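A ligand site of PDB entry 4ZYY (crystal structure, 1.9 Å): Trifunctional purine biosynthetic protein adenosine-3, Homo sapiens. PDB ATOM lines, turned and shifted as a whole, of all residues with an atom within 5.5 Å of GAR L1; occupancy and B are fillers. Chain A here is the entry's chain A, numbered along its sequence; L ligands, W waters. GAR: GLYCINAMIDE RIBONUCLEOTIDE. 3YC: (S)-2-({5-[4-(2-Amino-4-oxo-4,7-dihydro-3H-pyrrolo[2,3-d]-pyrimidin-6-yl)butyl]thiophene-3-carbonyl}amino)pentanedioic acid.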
ATOM      1  N   GLY A  10     -11.399   2.627  22.793  1.00  0.00           N
ATOM      2  CA  GLY A  10     -10.263   2.310  23.650  1.00  0.00           C
ATOM      3  C   GLY A  10     -10.461   1.248  24.713  1.00  0.00           C
ATOM      4  O   GLY A  10     -10.884   0.130  24.417  1.00  0.00           O
ATOM      5  N   THR A  11     -10.139   1.609  25.963  1.00  0.00           N
ATOM      6  CA  THR A  11     -10.038   0.671  27.090  1.00  0.00           C
ATOM      7  C   THR A  11     -11.305  -0.138  27.357  1.00  0.00           C
ATOM      8  O   THR A  11     -11.254  -1.352  27.557  1.00  0.00           O
ATOM      9  CB  THR A  11      -9.650   1.428  28.390  1.00  0.00           C
ATOM     10  OG1 THR A  11      -8.392   2.074  28.213  1.00  0.00           O
ATOM     11  CG2 THR A  11      -9.581   0.469  29.568  1.00  0.00           C
ATOM     12  N   GLY A  12     -12.447   0.539  27.382  1.00  0.00           N
ATOM     13  CA  GLY A  12     -13.722  -0.127  27.520  1.00  0.00           C
ATOM     14  C   GLY A  12     -14.169  -0.390  28.952  1.00  0.00           C
ATOM     15  O   GLY A  12     -14.939  -1.324  29.175  1.00  0.00           O
ATOM     16  N   SER A  13     -13.726   0.418  29.919  1.00  0.00           N
ATOM     17  CA  SER A  13     -14.222   0.243  31.288  1.00  0.00           C
ATOM     18  C   SER A  13     -15.720   0.561  31.369  1.00  0.00           C
ATOM     19  O   SER A  13     -16.472  -0.117  32.080  1.00  0.00           O
ATOM     20  CB  SER A  13     -13.440   1.091  32.297  1.00  0.00           C
ATOM     21  OG  SER A  13     -13.749   2.464  32.167  1.00  0.00           O
ATOM     22  N   ASN A  14     -16.164   1.572  30.632  1.00  0.00           N
ATOM     23  CA  ASN A  14     -17.597   1.853  30.579  1.00  0.00           C
ATOM     24  C   ASN A  14     -18.372   0.722  29.897  1.00  0.00           C
ATOM     25  O   ASN A  14     -19.435   0.342  30.380  1.00  0.00           O
ATOM     26  CB  ASN A  14     -17.870   3.182  29.867  1.00  0.00           C
ATOM     27  CG  ASN A  14     -17.824   4.364  30.824  1.00  0.00           C
ATOM     28  OD1 ASN A  14     -18.691   4.521  31.673  1.00  0.00           O
ATOM     29  ND2 ASN A  14     -16.798   5.186  30.695  1.00  0.00           N
ATOM     30  N   LEU A  15     -17.837   0.195  28.806  1.00  0.00           N
ATOM     31  CA  LEU A  15     -18.420  -0.998  28.187  1.00  0.00           C
ATOM     32  C   LEU A  15     -18.562  -2.145  29.180  1.00  0.00           C
ATOM     33  O   LEU A  15     -19.607  -2.790  29.236  1.00  0.00           O
ATOM     34  CB  LEU A  15     -17.563  -1.464  27.001  1.00  0.00           C
ATOM     35  CG  LEU A  15     -17.862  -2.876  26.478  1.00  0.00           C
ATOM     36  CD1 LEU A  15     -19.289  -2.955  25.876  1.00  0.00           C
ATOM     37  CD2 LEU A  15     -16.830  -3.301  25.427  1.00  0.00           C
ATOM     38  N   ALA A  87     -19.374   4.853  24.315  1.00  0.00           N
ATOM     39  CA  ALA A  87     -18.667   4.552  25.563  1.00  0.00           C
ATOM     40  C   ALA A  87     -17.165   4.686  25.348  1.00  0.00           C
ATOM     41  O   ALA A  87     -16.478   3.698  25.067  1.00  0.00           O
ATOM     42  CB  ALA A  87     -19.019   3.144  26.038  1.00  0.00           C
ATOM     43  N   GLY A  88     -16.655   5.909  25.462  1.00  0.00           N
ATOM     44  CA  GLY A  88     -15.268   6.213  25.146  1.00  0.00           C
ATOM     45  C   GLY A  88     -15.044   6.225  23.643  1.00  0.00           C
ATOM     46  O   GLY A  88     -13.907   6.127  23.185  1.00  0.00           O
ATOM     47  N   PHE A  89     -16.127   6.330  22.874  1.00  0.00           N
ATOM     48  CA  PHE A  89     -16.039   6.505  21.420  1.00  0.00           C
ATOM     49  C   PHE A  89     -15.693   7.957  21.127  1.00  0.00           C
ATOM     50  O   PHE A  89     -16.414   8.866  21.534  1.00  0.00           O
ATOM     51  CB  PHE A  89     -17.368   6.113  20.769  1.00  0.00           C
ATOM     52  CG  PHE A  89     -17.362   6.174  19.267  1.00  0.00           C
ATOM     53  CD1 PHE A  89     -16.761   5.181  18.515  1.00  0.00           C
ATOM     54  CD2 PHE A  89     -18.023   7.209  18.612  1.00  0.00           C
ATOM     55  CE1 PHE A  89     -16.794   5.215  17.125  1.00  0.00           C
ATOM     56  CE2 PHE A  89     -18.067   7.251  17.220  1.00  0.00           C
ATOM     57  CZ  PHE A  89     -17.447   6.261  16.473  1.00  0.00           C
ATOM     58  N   MET A  90     -14.583   8.192  20.417  1.00  0.00           N
ATOM     59  CA  MET A  90     -14.060   9.558  20.325  1.00  0.00           C
ATOM     60  C   MET A  90     -14.221  10.239  18.969  1.00  0.00           C
ATOM     61  O   MET A  90     -13.478  11.177  18.656  1.00  0.00           O
ATOM     62  CB  MET A  90     -12.571   9.565  20.714  1.00  0.00           C
ATOM     63  CG  MET A  90     -12.268   9.149  22.154  1.00  0.00           C
ATOM     64  SD  MET A  90     -13.193  10.055  23.434  1.00  0.00           S
ATOM     65  CE  MET A  90     -12.569  11.720  23.181  1.00  0.00           C
ATOM     66  N   ASN A 107     -24.471   9.259  25.242  1.00  0.00           N
ATOM     67  CA  ASN A 107     -23.032   9.465  25.354  1.00  0.00           C
ATOM     68  C   ASN A 107     -22.653   9.717  26.801  1.00  0.00           C
ATOM     69  O   ASN A 107     -23.428  10.342  27.530  1.00  0.00           O
ATOM     70  CB  ASN A 107     -22.568  10.633  24.479  1.00  0.00           C
ATOM     71  CG  ASN A 107     -21.072  10.880  24.590  1.00  0.00           C
ATOM     72  OD1 ASN A 107     -20.272   9.986  24.300  1.00  0.00           O
ATOM     73  ND2 ASN A 107     -20.685  12.094  24.995  1.00  0.00           N
ATOM     74  N   ILE A 108     -21.481   9.230  27.227  1.00  0.00           N
ATOM     75  CA  ILE A 108     -20.937   9.526  28.547  1.00  0.00           C
ATOM     76  C   ILE A 108     -19.827  10.552  28.373  1.00  0.00           C
ATOM     77  O   ILE A 108     -18.973  10.448  27.466  1.00  0.00           O
ATOM     78  CB  ILE A 108     -20.409   8.253  29.291  1.00  0.00           C
ATOM     79  CG1 ILE A 108     -19.874   8.590  30.696  1.00  0.00           C
ATOM     80  CG2 ILE A 108     -19.306   7.573  28.515  1.00  0.00           C
ATOM     81  CD1 ILE A 108     -20.945   8.681  31.743  1.00  0.00           C
ATOM     82  N   HIS A 109     -19.877  11.594  29.192  1.00  0.00           N
ATOM     83  CA  HIS A 109     -18.900  12.667  29.126  1.00  0.00           C
ATOM     84  C   HIS A 109     -18.365  12.965  30.516  1.00  0.00           C
ATOM     85  O   HIS A 109     -19.148  13.089  31.455  1.00  0.00           O
ATOM     86  CB  HIS A 109     -19.523  13.910  28.510  1.00  0.00           C
ATOM     87  CG  HIS A 109     -18.566  15.047  28.364  1.00  0.00           C
ATOM     88  ND1 HIS A 109     -17.675  15.147  27.317  1.00  0.00           N
ATOM     89  CD2 HIS A 109     -18.337  16.126  29.146  1.00  0.00           C
ATOM     90  CE1 HIS A 109     -16.949  16.246  27.449  1.00  0.00           C
ATOM     91  NE2 HIS A 109     -17.343  16.861  28.547  1.00  0.00           N
ATOM     92  N   PRO A 110     -17.024  13.056  30.670  1.00  0.00           N
ATOM     93  CA  PRO A 110     -16.406  13.161  31.992  1.00  0.00           C
ATOM     94  C   PRO A 110     -16.330  14.591  32.512  1.00  0.00           C
ATOM     95  O   PRO A 110     -15.276  15.039  32.984  1.00  0.00           O
ATOM     96  CB  PRO A 110     -15.008  12.572  31.754  1.00  0.00           C
ATOM     97  CG  PRO A 110     -14.691  12.980  30.360  1.00  0.00           C
ATOM     98  CD  PRO A 110     -16.007  12.875  29.607  1.00  0.00           C
ATOM     99  N   GLY A 118     -15.994  18.908  25.074  1.00  0.00           N
ATOM    100  CA  GLY A 118     -14.842  18.589  24.246  1.00  0.00           C
ATOM    101  C   GLY A 118     -14.095  17.345  24.686  1.00  0.00           C
ATOM    102  O   GLY A 118     -14.560  16.587  25.544  1.00  0.00           O
ATOM    103  N   SER A 119     -12.926  17.130  24.106  1.00  0.00           N
ATOM    104  CA  SER A 119     -12.260  15.837  24.226  1.00  0.00           C
ATOM    105  C   SER A 119     -11.267  15.764  25.372  1.00  0.00           C
ATOM    106  O   SER A 119     -10.720  14.691  25.637  1.00  0.00           O
ATOM    107  CB  SER A 119     -11.548  15.507  22.917  1.00  0.00           C
ATOM    108  OG  SER A 119     -10.552  16.474  22.695  1.00  0.00           O
ATOM    109  N   HIS A 122     -10.993  16.652  31.561  1.00  0.00           N
ATOM    110  CA  HIS A 122     -10.221  16.661  32.806  1.00  0.00           C
ATOM    111  C   HIS A 122      -9.144  17.738  32.788  1.00  0.00           C
ATOM    112  O   HIS A 122      -8.943  18.425  33.790  1.00  0.00           O
ATOM    113  CB  HIS A 122      -9.583  15.288  33.075  1.00  0.00           C
ATOM    114  CG  HIS A 122     -10.586  14.187  33.287  1.00  0.00           C
ATOM    115  ND1 HIS A 122     -11.572  14.251  34.237  1.00  0.00           N
ATOM    116  CD2 HIS A 122     -10.746  13.006  32.654  1.00  0.00           C
ATOM    117  CE1 HIS A 122     -12.301  13.154  34.188  1.00  0.00           C
ATOM    118  NE2 HIS A 122     -11.818  12.369  33.246  1.00  0.00           N
ATOM    119  N   ASP A 145     -21.817  17.512  22.747  1.00  0.00           N
ATOM    120  CA  ASP A 145     -21.987  17.648  24.192  1.00  0.00           C
ATOM    121  C   ASP A 145     -23.076  18.652  24.579  1.00  0.00           C
ATOM    122  O   ASP A 145     -23.039  19.228  25.668  1.00  0.00           O
ATOM    123  CB  ASP A 145     -20.655  18.029  24.874  1.00  0.00           C
ATOM    124  CG  ASP A 145     -19.573  16.965  24.696  1.00  0.00           C
ATOM    125  OD1 ASP A 145     -19.917  15.785  24.454  1.00  0.00           O
ATOM    126  OD2 ASP A 145     -18.384  17.308  24.793  1.00  0.00           O
ATOM    127  N   LYS A 171     -14.282   7.952  36.706  1.00  0.00           N
ATOM    128  CA  LYS A 171     -14.730   6.718  36.044  1.00  0.00           C
ATOM    129  C   LYS A 171     -15.566   5.851  36.978  1.00  0.00           C
ATOM    130  O   LYS A 171     -16.471   5.144  36.540  1.00  0.00           O
ATOM    131  CB  LYS A 171     -13.535   5.923  35.495  1.00  0.00           C
ATOM    132  CG  LYS A 171     -13.077   6.419  34.108  1.00  0.00           C
ATOM    133  CD  LYS A 171     -12.091   5.449  33.470  1.00  0.00           C
ATOM    134  CE  LYS A 171     -11.621   5.916  32.093  1.00  0.00           C
ATOM    135  NZ  LYS A 171     -10.688   4.924  31.470  1.00  0.00           N
ATOM    136  N   GLU A 174     -18.922   7.278  36.425  1.00  0.00           N
ATOM    137  CA  GLU A 174     -19.372   6.944  35.052  1.00  0.00           C
ATOM    138  C   GLU A 174     -19.974   5.553  35.026  1.00  0.00           C
ATOM    139  O   GLU A 174     -20.997   5.320  34.393  1.00  0.00           O
ATOM    140  CB  GLU A 174     -18.223   7.009  34.047  1.00  0.00           C
ATOM    141  CG  GLU A 174     -17.609   8.381  33.854  1.00  0.00           C
ATOM    142  CD  GLU A 174     -16.457   8.363  32.849  1.00  0.00           C
ATOM    143  OE1 GLU A 174     -16.505   7.581  31.884  1.00  0.00           O
ATOM    144  OE2 GLU A 174     -15.493   9.128  33.008  1.00  0.00           O
ATOM    145  N   HIS A 175     -19.312   4.627  35.728  1.00  0.00           N
ATOM    146  CA  HIS A 175     -19.735   3.237  35.738  1.00  0.00           C
ATOM    147  C   HIS A 175     -21.031   3.023  36.497  1.00  0.00           C
ATOM    148  O   HIS A 175     -21.621   1.955  36.425  1.00  0.00           O
ATOM    149  CB  HIS A 175     -18.651   2.350  36.336  1.00  0.00           C
ATOM    150  CG  HIS A 175     -17.377   2.376  35.577  1.00  0.00           C
ATOM    151  ND1 HIS A 175     -16.182   1.946  36.111  1.00  0.00           N
ATOM    152  CD2 HIS A 175     -17.100   2.795  34.320  1.00  0.00           C
ATOM    153  CE1 HIS A 175     -15.224   2.086  35.212  1.00  0.00           C
ATOM    154  NE2 HIS A 175     -15.756   2.602  34.113  1.00  0.00           N
HETATM  155  C1  GAR L   1     -14.354   7.884  29.765  1.00  0.00           C
HETATM  156  O6  GAR L   1     -13.870   8.636  30.882  1.00  0.00           O
HETATM  157  C2  GAR L   1     -15.317   8.757  29.009  1.00  0.00           C
HETATM  158  O8  GAR L   1     -16.077   9.610  29.847  1.00  0.00           O
HETATM  159  C3  GAR L   1     -14.386   9.585  28.136  1.00  0.00           C
HETATM  160  O4  GAR L   1     -13.389   8.647  27.735  1.00  0.00           O
HETATM  161  C5  GAR L   1     -13.224   7.668  28.769  1.00  0.00           C
HETATM  162  C10 GAR L   1     -13.302   6.276  28.160  1.00  0.00           C
HETATM  163  O12 GAR L   1     -12.973   5.263  29.117  1.00  0.00           O
HETATM  164  N19 GAR L   1     -15.106  10.128  27.012  1.00  0.00           N
HETATM  165  C21 GAR L   1     -14.923  11.376  26.596  1.00  0.00           C
HETATM  166  O22 GAR L   1     -14.047  12.118  27.042  1.00  0.00           O
HETATM  167  C23 GAR L   1     -15.875  11.799  25.510  1.00  0.00           C
HETATM  168  N24 GAR L   1     -15.810  13.224  25.254  1.00  0.00           N
HETATM  169  P15 GAR L   1     -13.333   3.715  28.851  1.00  0.00           P
HETATM  170  O16 GAR L   1     -14.833   3.721  28.867  1.00  0.00           O
HETATM  171  O17 GAR L   1     -12.627   2.995  29.978  1.00  0.00           O
HETATM  172  O18 GAR L   1     -12.768   3.373  27.471  1.00  0.00           O
HETATM  173  N1  3YC L   2     -21.146  13.665  17.866  1.00  0.00           N
HETATM  174  C2  3YC L   2     -22.096  14.595  17.882  1.00  0.00           C
HETATM  175  N3  3YC L   2     -22.596  15.030  19.053  1.00  0.00           N
HETATM  176  C4  3YC L   2     -22.159  14.560  20.238  1.00  0.00           C
HETATM  177  N5  3YC L   2     -19.734  12.233  19.225  1.00  0.00           N
HETATM  178  C6  3YC L   2     -19.579  12.034  20.541  1.00  0.00           C
HETATM  179  C7  3YC L   2     -20.459  12.857  21.228  1.00  0.00           C
HETATM  180  C8  3YC L   2     -21.164  13.586  20.238  1.00  0.00           C
HETATM  181  C9  3YC L   2     -20.668  13.156  19.005  1.00  0.00           C
HETATM  182  O10 3YC L   2     -22.634  15.000  21.280  1.00  0.00           O
HETATM  183  N11 3YC L   2     -22.593  15.129  16.648  1.00  0.00           N
HETATM  184  C12 3YC L   2     -14.321  14.062  20.034  1.00  0.00           C
HETATM  185  C13 3YC L   2     -13.861  15.239  19.389  1.00  0.00           C
HETATM  186  C14 3YC L   2     -14.265  16.412  19.936  1.00  0.00           C
HETATM  187  S15 3YC L   2     -15.229  15.985  21.283  1.00  0.00           S
HETATM  188  C16 3YC L   2     -15.092  14.298  21.127  1.00  0.00           C
HETATM  189  C17 3YC L   2     -13.048  15.163  18.204  1.00  0.00           C
HETATM  190  O18 3YC L   2     -12.534  16.180  17.759  1.00  0.00           O
HETATM  191  N19 3YC L   2     -12.875  13.893  17.562  1.00  0.00           N
HETATM  192  C20 3YC L   2     -12.138  13.725  16.439  1.00  0.00           C
HETATM  193  C21 3YC L   2     -11.531  12.438  16.471  1.00  0.00           C
HETATM  194  C22 3YC L   2     -10.161  12.518  17.048  1.00  0.00           C
HETATM  195  C23 3YC L   2      -9.758  11.155  17.507  1.00  0.00           C
HETATM  196  O24 3YC L   2      -9.800  10.174  16.714  1.00  0.00           O
HETATM  197  O25 3YC L   2      -9.372  10.981  18.699  1.00  0.00           O
HETATM  198  C26 3YC L   2     -12.969  13.778  15.291  1.00  0.00           C
HETATM  199  O27 3YC L   2     -12.577  14.424  14.273  1.00  0.00           O
HETATM  200  O28 3YC L   2     -14.083  13.199  15.254  1.00  0.00           O
HETATM  201  C29 3YC L   2     -18.621  11.072  21.148  1.00  0.00           C
HETATM  202  C30 3YC L   2     -17.675  11.833  22.000  1.00  0.00           C
HETATM  203  C31 3YC L   2     -16.692  12.528  21.133  1.00  0.00           C
HETATM  204  C32 3YC L   2     -15.709  13.255  21.990  1.00  0.00           C
HETATM  205  O   HOH W   1     -10.609   4.579  26.386  1.00  0.00           O
HETATM  206  O   HOH W   2     -17.353   8.701  26.125  1.00  0.00           O
HETATM  207  O   HOH W   3     -13.710   3.125  24.741  1.00  0.00           O
HETATM  208  O   HOH W   4     -11.649   9.902  31.104  1.00  0.00           O
HETATM  209  O   HOH W   5     -18.164  13.826  24.995  1.00  0.00           O
HETATM  210  O   HOH W   6     -16.051   1.976  27.214  1.00  0.00           O
HETATM  211  O   HOH W   7     -13.103   9.941  33.754  1.00  0.00           O
HETATM  212  O   HOH W   8     -13.373  14.808  27.568  1.00  0.00           O
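Thr 11 touches GAR L1. Gly 88 touches GAR L1 (CA to C10, 3.6 Å). Met 90 touches GAR L1 (SD to C23, 3.8 Å). Ile 108 touches GAR L1 (O to O8, 3.8 Å). Pro 110 touches GAR L1 (CD to O8, 3.3 Å). Gly 118 touches GAR L1. Of the 21 residues printed, 12 come within 4 Å of GAR L1.
The backbone NH of Ser 13 lies within hydrogen-bond range of an oxygen (O17) of GAR L1 (2.8 Å). The side-chain hydroxyl (OG) of Ser 13 lies within hydrogen-bond range of an oxygen (O17) of GAR L1, 2.5 Å away. OE2 of Glu 174 is in hydrogen-bond range of O6 of GAR L1 (2.7 Å). An oxygen (O18) of GAR L1 is in hydrogen-bond range of the backbone NH (N) of Gly 12 (2.9 Å). O16 of GAR L1 is in hydrogen-bond range of N of Asn 14 (3.1 Å). The side-chain amide nitrogen (ND2) of Asn 14 is in hydrogen-bond range of an oxygen (O16) of GAR L1. An oxygen (O17) of GAR L1 is in salt-bridge range of the side-chain amino group (NZ) of Lys 171 (3.1 Å). A ring nitrogen (ND1) of His 109 lies within hydrogen-bond range of a nitrogen (N24) of GAR L1 (3.4 Å). O of Met 90 is in hydrogen-bond range of N19 of 3YC L2 (3.0 Å). An oxygen (O10) of 3YC L2 is in hydrogen-bond range of the backbone NH of Asp 145 (3.0 Å).
The side-chain hydroxyl of Ser 13 sits at hydrogen-bond distance from a ring nitrogen (NE2) of His 175 (2.8 Å). The side-chain amide nitrogen (ND2) of Asn 14 lies within hydrogen-bond range of the side-chain carboxylate (OE1) of Glu 174, at 2.7 Å. The backbone carbonyl oxygen (O) of Lys 171 lies close to a ring nitrogen (ND1) of His 175 (3.2 Å). A ring nitrogen (ND1) of His 109 sits close to the side-chain carboxylate (OD2) of Asp 145 (3.4 Å). N of Gly 118 is in hydrogen-bond range of OD2 of Asp 145.
Water W5 lies within hydrogen-bond range of a nitrogen (N24) of GAR L1 (2.4 Å), the side-chain carboxylate (OD1) of Asp 145 (2.7 Å), a ring nitrogen (ND1) of His 109 (2.7 Å) and the side-chain amide nitrogen (ND2) of Asn 107 (3.1 Å). Water W6 lies within hydrogen-bond range of O16 of GAR L1, O of Ala 87, N of Leu 15 and N of Asn 14. Water W1 lies within hydrogen-bond range of O18 of GAR L1 (2.7 Å) and N of Thr 11 (3.0 Å). Water W2 lies within hydrogen-bond range of the backbone carbonyl oxygen of Ile 108, a nitrogen (N19) of GAR L1 and the backbone NH of Gly 88. Water W3 lies within hydrogen-bond range of O of Ala 87 (2.8 Å), O18 of GAR L1 (2.9 Å), N of Gly 10 (3.1 Å) and O of Gly 88 (3.4 Å). Water W7 lies within hydrogen-bond range of the side-chain carboxylate (OE2) of Glu 174, a ring nitrogen (NE2) of His 122 and an oxygen (O6) of GAR L1.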
